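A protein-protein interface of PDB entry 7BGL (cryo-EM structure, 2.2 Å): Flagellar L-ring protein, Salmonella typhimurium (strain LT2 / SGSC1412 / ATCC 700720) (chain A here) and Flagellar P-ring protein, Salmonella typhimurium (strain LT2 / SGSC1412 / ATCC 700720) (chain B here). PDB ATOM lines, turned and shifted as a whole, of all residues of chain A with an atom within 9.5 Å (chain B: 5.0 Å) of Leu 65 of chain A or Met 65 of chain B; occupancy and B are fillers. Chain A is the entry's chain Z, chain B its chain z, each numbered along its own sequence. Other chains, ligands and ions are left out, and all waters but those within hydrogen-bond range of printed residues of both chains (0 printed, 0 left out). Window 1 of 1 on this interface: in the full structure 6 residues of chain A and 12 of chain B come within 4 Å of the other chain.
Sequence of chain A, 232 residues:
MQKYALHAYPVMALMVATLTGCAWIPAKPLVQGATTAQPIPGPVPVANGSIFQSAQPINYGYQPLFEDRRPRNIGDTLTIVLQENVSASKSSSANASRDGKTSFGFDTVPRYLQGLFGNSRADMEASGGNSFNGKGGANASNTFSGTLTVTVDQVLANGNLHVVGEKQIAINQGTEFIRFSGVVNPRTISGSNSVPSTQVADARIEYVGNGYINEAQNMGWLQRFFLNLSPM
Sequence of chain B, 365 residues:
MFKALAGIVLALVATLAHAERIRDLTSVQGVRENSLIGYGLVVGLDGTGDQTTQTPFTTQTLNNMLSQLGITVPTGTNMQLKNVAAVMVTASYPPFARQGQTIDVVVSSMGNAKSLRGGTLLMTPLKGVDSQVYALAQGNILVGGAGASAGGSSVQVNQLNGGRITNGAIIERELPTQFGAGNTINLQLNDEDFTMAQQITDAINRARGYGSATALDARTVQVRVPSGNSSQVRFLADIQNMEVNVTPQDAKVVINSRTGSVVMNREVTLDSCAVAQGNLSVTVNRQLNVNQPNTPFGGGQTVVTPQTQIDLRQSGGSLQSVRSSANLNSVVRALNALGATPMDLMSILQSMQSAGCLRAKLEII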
ATOM      1  N   TYR A  62     -13.020  -5.516  12.851  1.00  0.00           N
ATOM      2  CA  TYR A  62     -14.375  -5.243  12.396  1.00  0.00           C
ATOM      3  C   TYR A  62     -15.263  -4.853  13.570  1.00  0.00           C
ATOM      4  O   TYR A  62     -15.154  -5.410  14.666  1.00  0.00           O
ATOM      5  CB  TYR A  62     -14.946  -6.468  11.683  1.00  0.00           C
ATOM      6  CG  TYR A  62     -16.455  -6.553  11.700  1.00  0.00           C
ATOM      7  CD1 TYR A  62     -17.222  -5.793  10.829  1.00  0.00           C
ATOM      8  CD2 TYR A  62     -17.111  -7.400  12.581  1.00  0.00           C
ATOM      9  CE1 TYR A  62     -18.600  -5.870  10.840  1.00  0.00           C
ATOM     10  CE2 TYR A  62     -18.488  -7.484  12.599  1.00  0.00           C
ATOM     11  CZ  TYR A  62     -19.227  -6.717  11.726  1.00  0.00           C
ATOM     12  OH  TYR A  62     -20.600  -6.798  11.740  1.00  0.00           O
ATOM     13  N   GLN A  63     -16.148  -3.887  13.337  1.00  0.00           N
ATOM     14  CA  GLN A  63     -17.048  -3.416  14.380  1.00  0.00           C
ATOM     15  C   GLN A  63     -18.465  -3.276  13.838  1.00  0.00           C
ATOM     16  O   GLN A  63     -18.695  -2.527  12.880  1.00  0.00           O
ATOM     17  CB  GLN A  63     -16.558  -2.082  14.946  1.00  0.00           C
ATOM     18  CG  GLN A  63     -15.217  -2.175  15.654  1.00  0.00           C
ATOM     19  CD  GLN A  63     -14.735  -0.834  16.169  1.00  0.00           C
ATOM     20  OE1 GLN A  63     -15.092   0.215  15.632  1.00  0.00           O
ATOM     21  NE2 GLN A  63     -13.921  -0.861  17.217  1.00  0.00           N
ATOM     22  N   PRO A  64     -19.437  -3.973  14.419  1.00  0.00           N
ATOM     23  CA  PRO A  64     -20.819  -3.849  13.947  1.00  0.00           C
ATOM     24  C   PRO A  64     -21.387  -2.470  14.243  1.00  0.00           C
ATOM     25  O   PRO A  64     -20.948  -1.762  15.152  1.00  0.00           O
ATOM     26  CB  PRO A  64     -21.565  -4.936  14.726  1.00  0.00           C
ATOM     27  CG  PRO A  64     -20.732  -5.189  15.931  1.00  0.00           C
ATOM     28  CD  PRO A  64     -19.309  -4.900  15.555  1.00  0.00           C
ATOM     29  N   LEU A  65     -22.386  -2.092  13.448  1.00  0.00           N
ATOM     30  CA  LEU A  65     -22.997  -0.776  13.571  1.00  0.00           C
ATOM     31  C   LEU A  65     -24.233  -0.778  14.461  1.00  0.00           C
ATOM     32  O   LEU A  65     -24.401   0.128  15.285  1.00  0.00           O
ATOM     33  CB  LEU A  65     -23.365  -0.234  12.188  1.00  0.00           C
ATOM     34  CG  LEU A  65     -22.214   0.225  11.294  1.00  0.00           C
ATOM     35  CD1 LEU A  65     -22.707   0.453   9.876  1.00  0.00           C
ATOM     36  CD2 LEU A  65     -21.571   1.484  11.850  1.00  0.00           C
ATOM     37  N   PHE A  66     -25.104  -1.776  14.318  1.00  0.00           N
ATOM     38  CA  PHE A  66     -26.392  -1.775  14.997  1.00  0.00           C
ATOM     39  C   PHE A  66     -26.401  -2.555  16.304  1.00  0.00           C
ATOM     40  O   PHE A  66     -27.417  -2.538  17.005  1.00  0.00           O
ATOM     41  CB  PHE A  66     -27.475  -2.335  14.066  1.00  0.00           C
ATOM     42  CG  PHE A  66     -27.513  -1.673  12.721  1.00  0.00           C
ATOM     43  CD1 PHE A  66     -27.846  -0.336  12.602  1.00  0.00           C
ATOM     44  CD2 PHE A  66     -27.212  -2.386  11.574  1.00  0.00           C
ATOM     45  CE1 PHE A  66     -27.880   0.278  11.368  1.00  0.00           C
ATOM     46  CE2 PHE A  66     -27.246  -1.778  10.335  1.00  0.00           C
ATOM     47  CZ  PHE A  66     -27.580  -0.445  10.233  1.00  0.00           C
ATOM     48  N   GLU A  67     -25.309  -3.228  16.655  1.00  0.00           N
ATOM     49  CA  GLU A  67     -25.284  -3.998  17.887  1.00  0.00           C
ATOM     50  C   GLU A  67     -25.057  -3.083  19.091  1.00  0.00           C
ATOM     51  O   GLU A  67     -24.673  -1.919  18.962  1.00  0.00           O
ATOM     52  CB  GLU A  67     -24.218  -5.088  17.814  1.00  0.00           C
ATOM     53  CG  GLU A  67     -24.362  -5.992  16.599  1.00  0.00           C
ATOM     54  CD  GLU A  67     -23.399  -7.161  16.618  1.00  0.00           C
ATOM     55  OE1 GLU A  67     -22.828  -7.481  15.554  1.00  0.00           O
ATOM     56  OE2 GLU A  67     -23.213  -7.763  17.696  1.00  0.00           O
ATOM     57  N   ASP A  68     -25.300  -3.634  20.281  1.00  0.00           N
ATOM     58  CA  ASP A  68     -25.332  -2.870  21.522  1.00  0.00           C
ATOM     59  C   ASP A  68     -23.948  -2.592  22.103  1.00  0.00           C
ATOM     60  O   ASP A  68     -23.856  -2.228  23.281  1.00  0.00           O
ATOM     61  CB  ASP A  68     -26.191  -3.595  22.561  1.00  0.00           C
ATOM     62  CG  ASP A  68     -27.643  -3.161  22.522  1.00  0.00           C
ATOM     63  OD1 ASP A  68     -27.931  -2.093  21.943  1.00  0.00           O
ATOM     64  OD2 ASP A  68     -28.497  -3.888  23.071  1.00  0.00           O
ATOM     65  N   ARG A  69     -22.884  -2.757  21.320  1.00  0.00           N
ATOM     66  CA  ARG A  69     -21.525  -2.432  21.759  1.00  0.00           C
ATOM     67  C   ARG A  69     -21.181  -3.116  23.081  1.00  0.00           C
ATOM     68  O   ARG A  69     -20.595  -2.517  23.985  1.00  0.00           O
ATOM     69  CB  ARG A  69     -21.324  -0.916  21.854  1.00  0.00           C
ATOM     70  CG  ARG A  69     -21.922  -0.252  23.086  1.00  0.00           C
ATOM     71  CD  ARG A  69     -21.639   1.241  23.091  1.00  0.00           C
ATOM     72  NE  ARG A  69     -22.294   1.925  24.200  1.00  0.00           N
ATOM     73  CZ  ARG A  69     -21.701   2.235  25.344  1.00  0.00           C
ATOM     74  NH1 ARG A  69     -20.434   1.931  25.571  1.00  0.00           N
ATOM     75  NH2 ARG A  69     -22.397   2.868  26.285  1.00  0.00           N
ATOM     76  N   ARG A  72     -16.309  -7.390  24.126  1.00  0.00           N
ATOM     77  CA  ARG A  72     -16.024  -8.587  23.345  1.00  0.00           C
ATOM     78  C   ARG A  72     -14.600  -9.103  23.476  1.00  0.00           C
ATOM     79  O   ARG A  72     -14.375 -10.289  23.211  1.00  0.00           O
ATOM     80  CB  ARG A  72     -16.319  -8.338  21.859  1.00  0.00           C
ATOM     81  CG  ARG A  72     -17.799  -8.306  21.525  1.00  0.00           C
ATOM     82  CD  ARG A  72     -18.032  -8.340  20.025  1.00  0.00           C
ATOM     83  NE  ARG A  72     -19.334  -7.791  19.667  1.00  0.00           N
ATOM     84  CZ  ARG A  72     -19.615  -6.496  19.629  1.00  0.00           C
ATOM     85  NH1 ARG A  72     -18.705  -5.582  19.920  1.00  0.00           N
ATOM     86  NH2 ARG A  72     -20.842  -6.108  19.291  1.00  0.00           N
ATOM     87  N   THR B  61     -31.164   0.937  17.753  1.00  0.00           N
ATOM     88  CA  THR B  61     -30.166   0.560  16.758  1.00  0.00           C
ATOM     89  C   THR B  61     -29.628   1.781  16.023  1.00  0.00           C
ATOM     90  O   THR B  61     -28.430   1.853  15.723  1.00  0.00           O
ATOM     91  CB  THR B  61     -30.760  -0.445  15.771  1.00  0.00           C
ATOM     92  OG1 THR B  61     -32.030   0.029  15.310  1.00  0.00           O
ATOM     93  CG2 THR B  61     -30.943  -1.794  16.443  1.00  0.00           C
ATOM     94  N   LEU B  62     -30.495   2.751  15.721  1.00  0.00           N
ATOM     95  CA  LEU B  62     -30.018   3.976  15.092  1.00  0.00           C
ATOM     96  C   LEU B  62     -29.048   4.716  16.003  1.00  0.00           C
ATOM     97  O   LEU B  62     -28.026   5.240  15.543  1.00  0.00           O
ATOM     98  CB  LEU B  62     -31.199   4.871  14.720  1.00  0.00           C
ATOM     99  CG  LEU B  62     -30.876   6.062  13.817  1.00  0.00           C
ATOM    100  CD1 LEU B  62     -31.913   6.198  12.717  1.00  0.00           C
ATOM    101  CD2 LEU B  62     -30.784   7.340  14.631  1.00  0.00           C
ATOM    102  N   ASN B  63     -29.350   4.770  17.302  1.00  0.00           N
ATOM    103  CA  ASN B  63     -28.444   5.410  18.248  1.00  0.00           C
ATOM    104  C   ASN B  63     -27.121   4.662  18.335  1.00  0.00           C
ATOM    105  O   ASN B  63     -26.056   5.280  18.436  1.00  0.00           O
ATOM    106  CB  ASN B  63     -29.100   5.502  19.624  1.00  0.00           C
ATOM    107  CG  ASN B  63     -30.076   6.655  19.726  1.00  0.00           C
ATOM    108  OD1 ASN B  63     -29.953   7.651  19.015  1.00  0.00           O
ATOM    109  ND2 ASN B  63     -31.055   6.525  20.613  1.00  0.00           N
ATOM    110  N   ASN B  64     -27.168   3.328  18.308  1.00  0.00           N
ATOM    111  CA  ASN B  64     -25.933   2.551  18.311  1.00  0.00           C
ATOM    112  C   ASN B  64     -25.090   2.863  17.083  1.00  0.00           C
ATOM    113  O   ASN B  64     -23.871   3.046  17.184  1.00  0.00           O
ATOM    114  CB  ASN B  64     -26.247   1.058  18.376  1.00  0.00           C
ATOM    115  CG  ASN B  64     -26.886   0.652  19.686  1.00  0.00           C
ATOM    116  OD1 ASN B  64     -26.785   1.361  20.685  1.00  0.00           O
ATOM    117  ND2 ASN B  64     -27.552  -0.496  19.687  1.00  0.00           N
ATOM    118  N   MET B  65     -25.725   2.928  15.912  1.00  0.00           N
ATOM    119  CA  MET B  65     -24.993   3.256  14.692  1.00  0.00           C
ATOM    120  C   MET B  65     -24.392   4.654  14.769  1.00  0.00           C
ATOM    121  O   MET B  65     -23.239   4.867  14.376  1.00  0.00           O
ATOM    122  CB  MET B  65     -25.913   3.133  13.480  1.00  0.00           C
ATOM    123  CG  MET B  65     -25.242   3.461  12.157  1.00  0.00           C
ATOM    124  SD  MET B  65     -26.427   3.772  10.837  1.00  0.00           S
ATOM    125  CE  MET B  65     -27.219   5.261  11.437  1.00  0.00           C
ATOM    126  N   LEU B  66     -25.160   5.621  15.275  1.00  0.00           N
ATOM    127  CA  LEU B  66     -24.646   6.981  15.396  1.00  0.00           C
ATOM    128  C   LEU B  66     -23.462   7.039  16.353  1.00  0.00           C
ATOM    129  O   LEU B  66     -22.463   7.713  16.077  1.00  0.00           O
ATOM    130  CB  LEU B  66     -25.757   7.923  15.858  1.00  0.00           C
ATOM    131  CG  LEU B  66     -26.794   8.324  14.808  1.00  0.00           C
ATOM    132  CD1 LEU B  66     -27.796   9.302  15.396  1.00  0.00           C
ATOM    133  CD2 LEU B  66     -26.118   8.916  13.585  1.00  0.00           C
ATOM    134  N   SER B  67     -23.556   6.344  17.488  1.00  0.00           N
ATOM    135  CA  SER B  67     -22.450   6.327  18.438  1.00  0.00           C
ATOM    136  C   SER B  67     -21.216   5.677  17.828  1.00  0.00           C
ATOM    137  O   SER B  67     -20.092   6.149  18.031  1.00  0.00           O
ATOM    138  CB  SER B  67     -22.864   5.604  19.718  1.00  0.00           C
ATOM    139  OG  SER B  67     -23.014   4.215  19.494  1.00  0.00           O
ATOM    140  N   GLN B  68     -21.406   4.593  17.077  1.00  0.00           N
ATOM    141  CA  GLN B  68     -20.274   3.962  16.405  1.00  0.00           C
ATOM    142  C   GLN B  68     -19.637   4.914  15.402  1.00  0.00           C
ATOM    143  O   GLN B  68     -18.408   4.973  15.285  1.00  0.00           O
ATOM    144  CB  GLN B  68     -20.723   2.674  15.716  1.00  0.00           C
ATOM    145  CG  GLN B  68     -19.685   2.084  14.781  1.00  0.00           C
ATOM    146  CD  GLN B  68     -18.457   1.586  15.515  1.00  0.00           C
ATOM    147  OE1 GLN B  68     -18.360   1.705  16.736  1.00  0.00           O
ATOM    148  NE2 GLN B  68     -17.511   1.027  14.774  1.00  0.00           N
ATOM    149  N   LEU B  69     -20.456   5.665  14.668  1.00  0.00           N
ATOM    150  CA  LEU B  69     -19.941   6.632  13.707  1.00  0.00           C
ATOM    151  C   LEU B  69     -19.313   7.851  14.368  1.00  0.00           C
ATOM    152  O   LEU B  69     -18.532   8.552  13.717  1.00  0.00           O
ATOM    153  CB  LEU B  69     -21.056   7.078  12.759  1.00  0.00           C
ATOM    154  CG  LEU B  69     -21.521   6.028  11.749  1.00  0.00           C
ATOM    155  CD1 LEU B  69     -22.731   6.523  10.974  1.00  0.00           C
ATOM    156  CD2 LEU B  69     -20.391   5.656  10.805  1.00  0.00           C
ATOM    157  N   LEU B 122     -28.362  -0.665   4.924  1.00  0.00           N
ATOM    158  CA  LEU B 122     -27.076  -0.130   5.362  1.00  0.00           C
ATOM    159  C   LEU B 122     -26.303  -1.196   6.131  1.00  0.00           C
ATOM    160  O   LEU B 122     -26.628  -1.489   7.286  1.00  0.00           O
ATOM    161  CB  LEU B 122     -27.280   1.105   6.237  1.00  0.00           C
ATOM    162  CG  LEU B 122     -28.115   2.259   5.687  1.00  0.00           C
ATOM    163  CD1 LEU B 122     -28.466   3.222   6.806  1.00  0.00           C
ATOM    164  CD2 LEU B 122     -27.374   2.976   4.577  1.00  0.00           C
ATOM    165  N   MET B 123     -25.294  -1.771   5.488  1.00  0.00           N
ATOM    166  CA  MET B 123     -24.230  -2.532   6.146  1.00  0.00           C
ATOM    167  C   MET B 123     -24.763  -3.428   7.265  1.00  0.00           C
ATOM    168  O   MET B 123     -24.427  -3.279   8.440  1.00  0.00           O
ATOM    169  CB  MET B 123     -23.148  -1.594   6.676  1.00  0.00           C
ATOM    170  CG  MET B 123     -21.872  -1.567   5.843  1.00  0.00           C
ATOM    171  SD  MET B 123     -21.288  -3.177   5.269  1.00  0.00           S
ATOM    172  CE  MET B 123     -21.759  -4.243   6.630  1.00  0.00           C
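Among the printed residues, pairs that only touch across the chains: Phe 66 of chain A with Leu 122 of chain B (3.1 Å), Leu 65 of chain A with Asn 64 of chain B (3.3 Å), Leu 65 of chain A with Gln 68 of chain B (3.5 Å), Phe 66 of chain A with Thr 61 of chain B (3.6 Å), Phe 66 of chain A with Met 123 of chain B (3.7 Å), Phe 66 of chain A with Met 65 of chain B (3.8 Å) and Leu 65 of chain A with Met 123 of chain B (3.8 Å).
Printed residues of chain A that touch a printed residue of chain B: Gln 63, Leu 65, Phe 66, Glu 67 and Asp 68.
Hydrophobic or aromatic side chains of chain A within 4 Å of the printed part of chain B: Leu 65 and Phe 66.
Of the 11 printed residues of chain B, 6 touch a printed residue of chain A.
Printed residues of chain B that touch a printed residue of chain A: Thr 61, Asn 64, Met 65, Gln 68, Leu 122 and Met 123.
Hydrophobic or aromatic side chains of chain B within 4 Å of the printed part of chain A: Met 65 and Met 123.
Along chain B the printed residues that touch a printed residue of chain A span positions 61 to 123.
OE2 of Glu 67 of chain A lies within salt-bridge range of NH2 of Arg 72 of chain A (3.3 Å).
O of Asn 64 of chain B sits at hydrogen-bond distance from OG of Ser 67 of chain B (2.7 Å).
NE2 of Gln 68 of chain B sits at hydrogen-bond distance from OE1 of Gln 63 of chain A, at 2.7 Å.
The backbone NH (N) of Met 65 of chain B sits at hydrogen-bond distance from the backbone carbonyl oxygen (O) of Leu 65 of chain A (3.2 Å).
The backbone carbonyl oxygen (O) of Phe 66 of chain A lies within hydrogen-bond range of the side-chain amide nitrogen (ND2) of Asn 64 of chain B, at 3.4 Å.
The side-chain amide nitrogen of Asn 64 of chain B lies within hydrogen-bond range of the backbone carbonyl oxygen of Glu 67 of chain A.
OD1 of Asp 68 of chain A is in hydrogen-bond range of ND2 of Asn 64 of chain B.
Tyr 62 of chain A touches none of the printed residues of chain B.
Printed residues of chain B within 4 Å of Leu 65 of chain A: Asn 64 (3.3 Å), Met 65 (3.2 Å), Gln 68 (3.5 Å) and Met 123 (3.8 Å).
Printed residues of chain B within 4 Å of Phe 66 of chain A: Thr 61 (3.6 Å), Asn 64 (3.4 Å), Met 65 (3.8 Å), Leu 122 (3.1 Å) and Met 123 (3.7 Å).
Of the printed residues of chain B, Asp 68 of chain A touches Asn 64.
Arg 72 of chain A touches none of the printed residues of chain B.
Of the printed residues of chain A, Thr 61 of chain B touches Phe 66.
Asn 64 of chain B touches four residues of chain A.
Of chain A, only Leu 65 and Phe 66 come within 4 Å of Met 65 of chain B.
No residue of chain A comes within 4 Å of Ser 67 of chain B.
Printed residues of chain A within 4 Å of Gln 68 of chain B: Gln 63 and Leu 65.
Printed residues of chain A within 4 Å of Leu 122 of chain B: Phe 66.
The nearest residue of chain B that does not touch Leu 65 of chain A is Thr 61 of chain B (4.4 Å).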
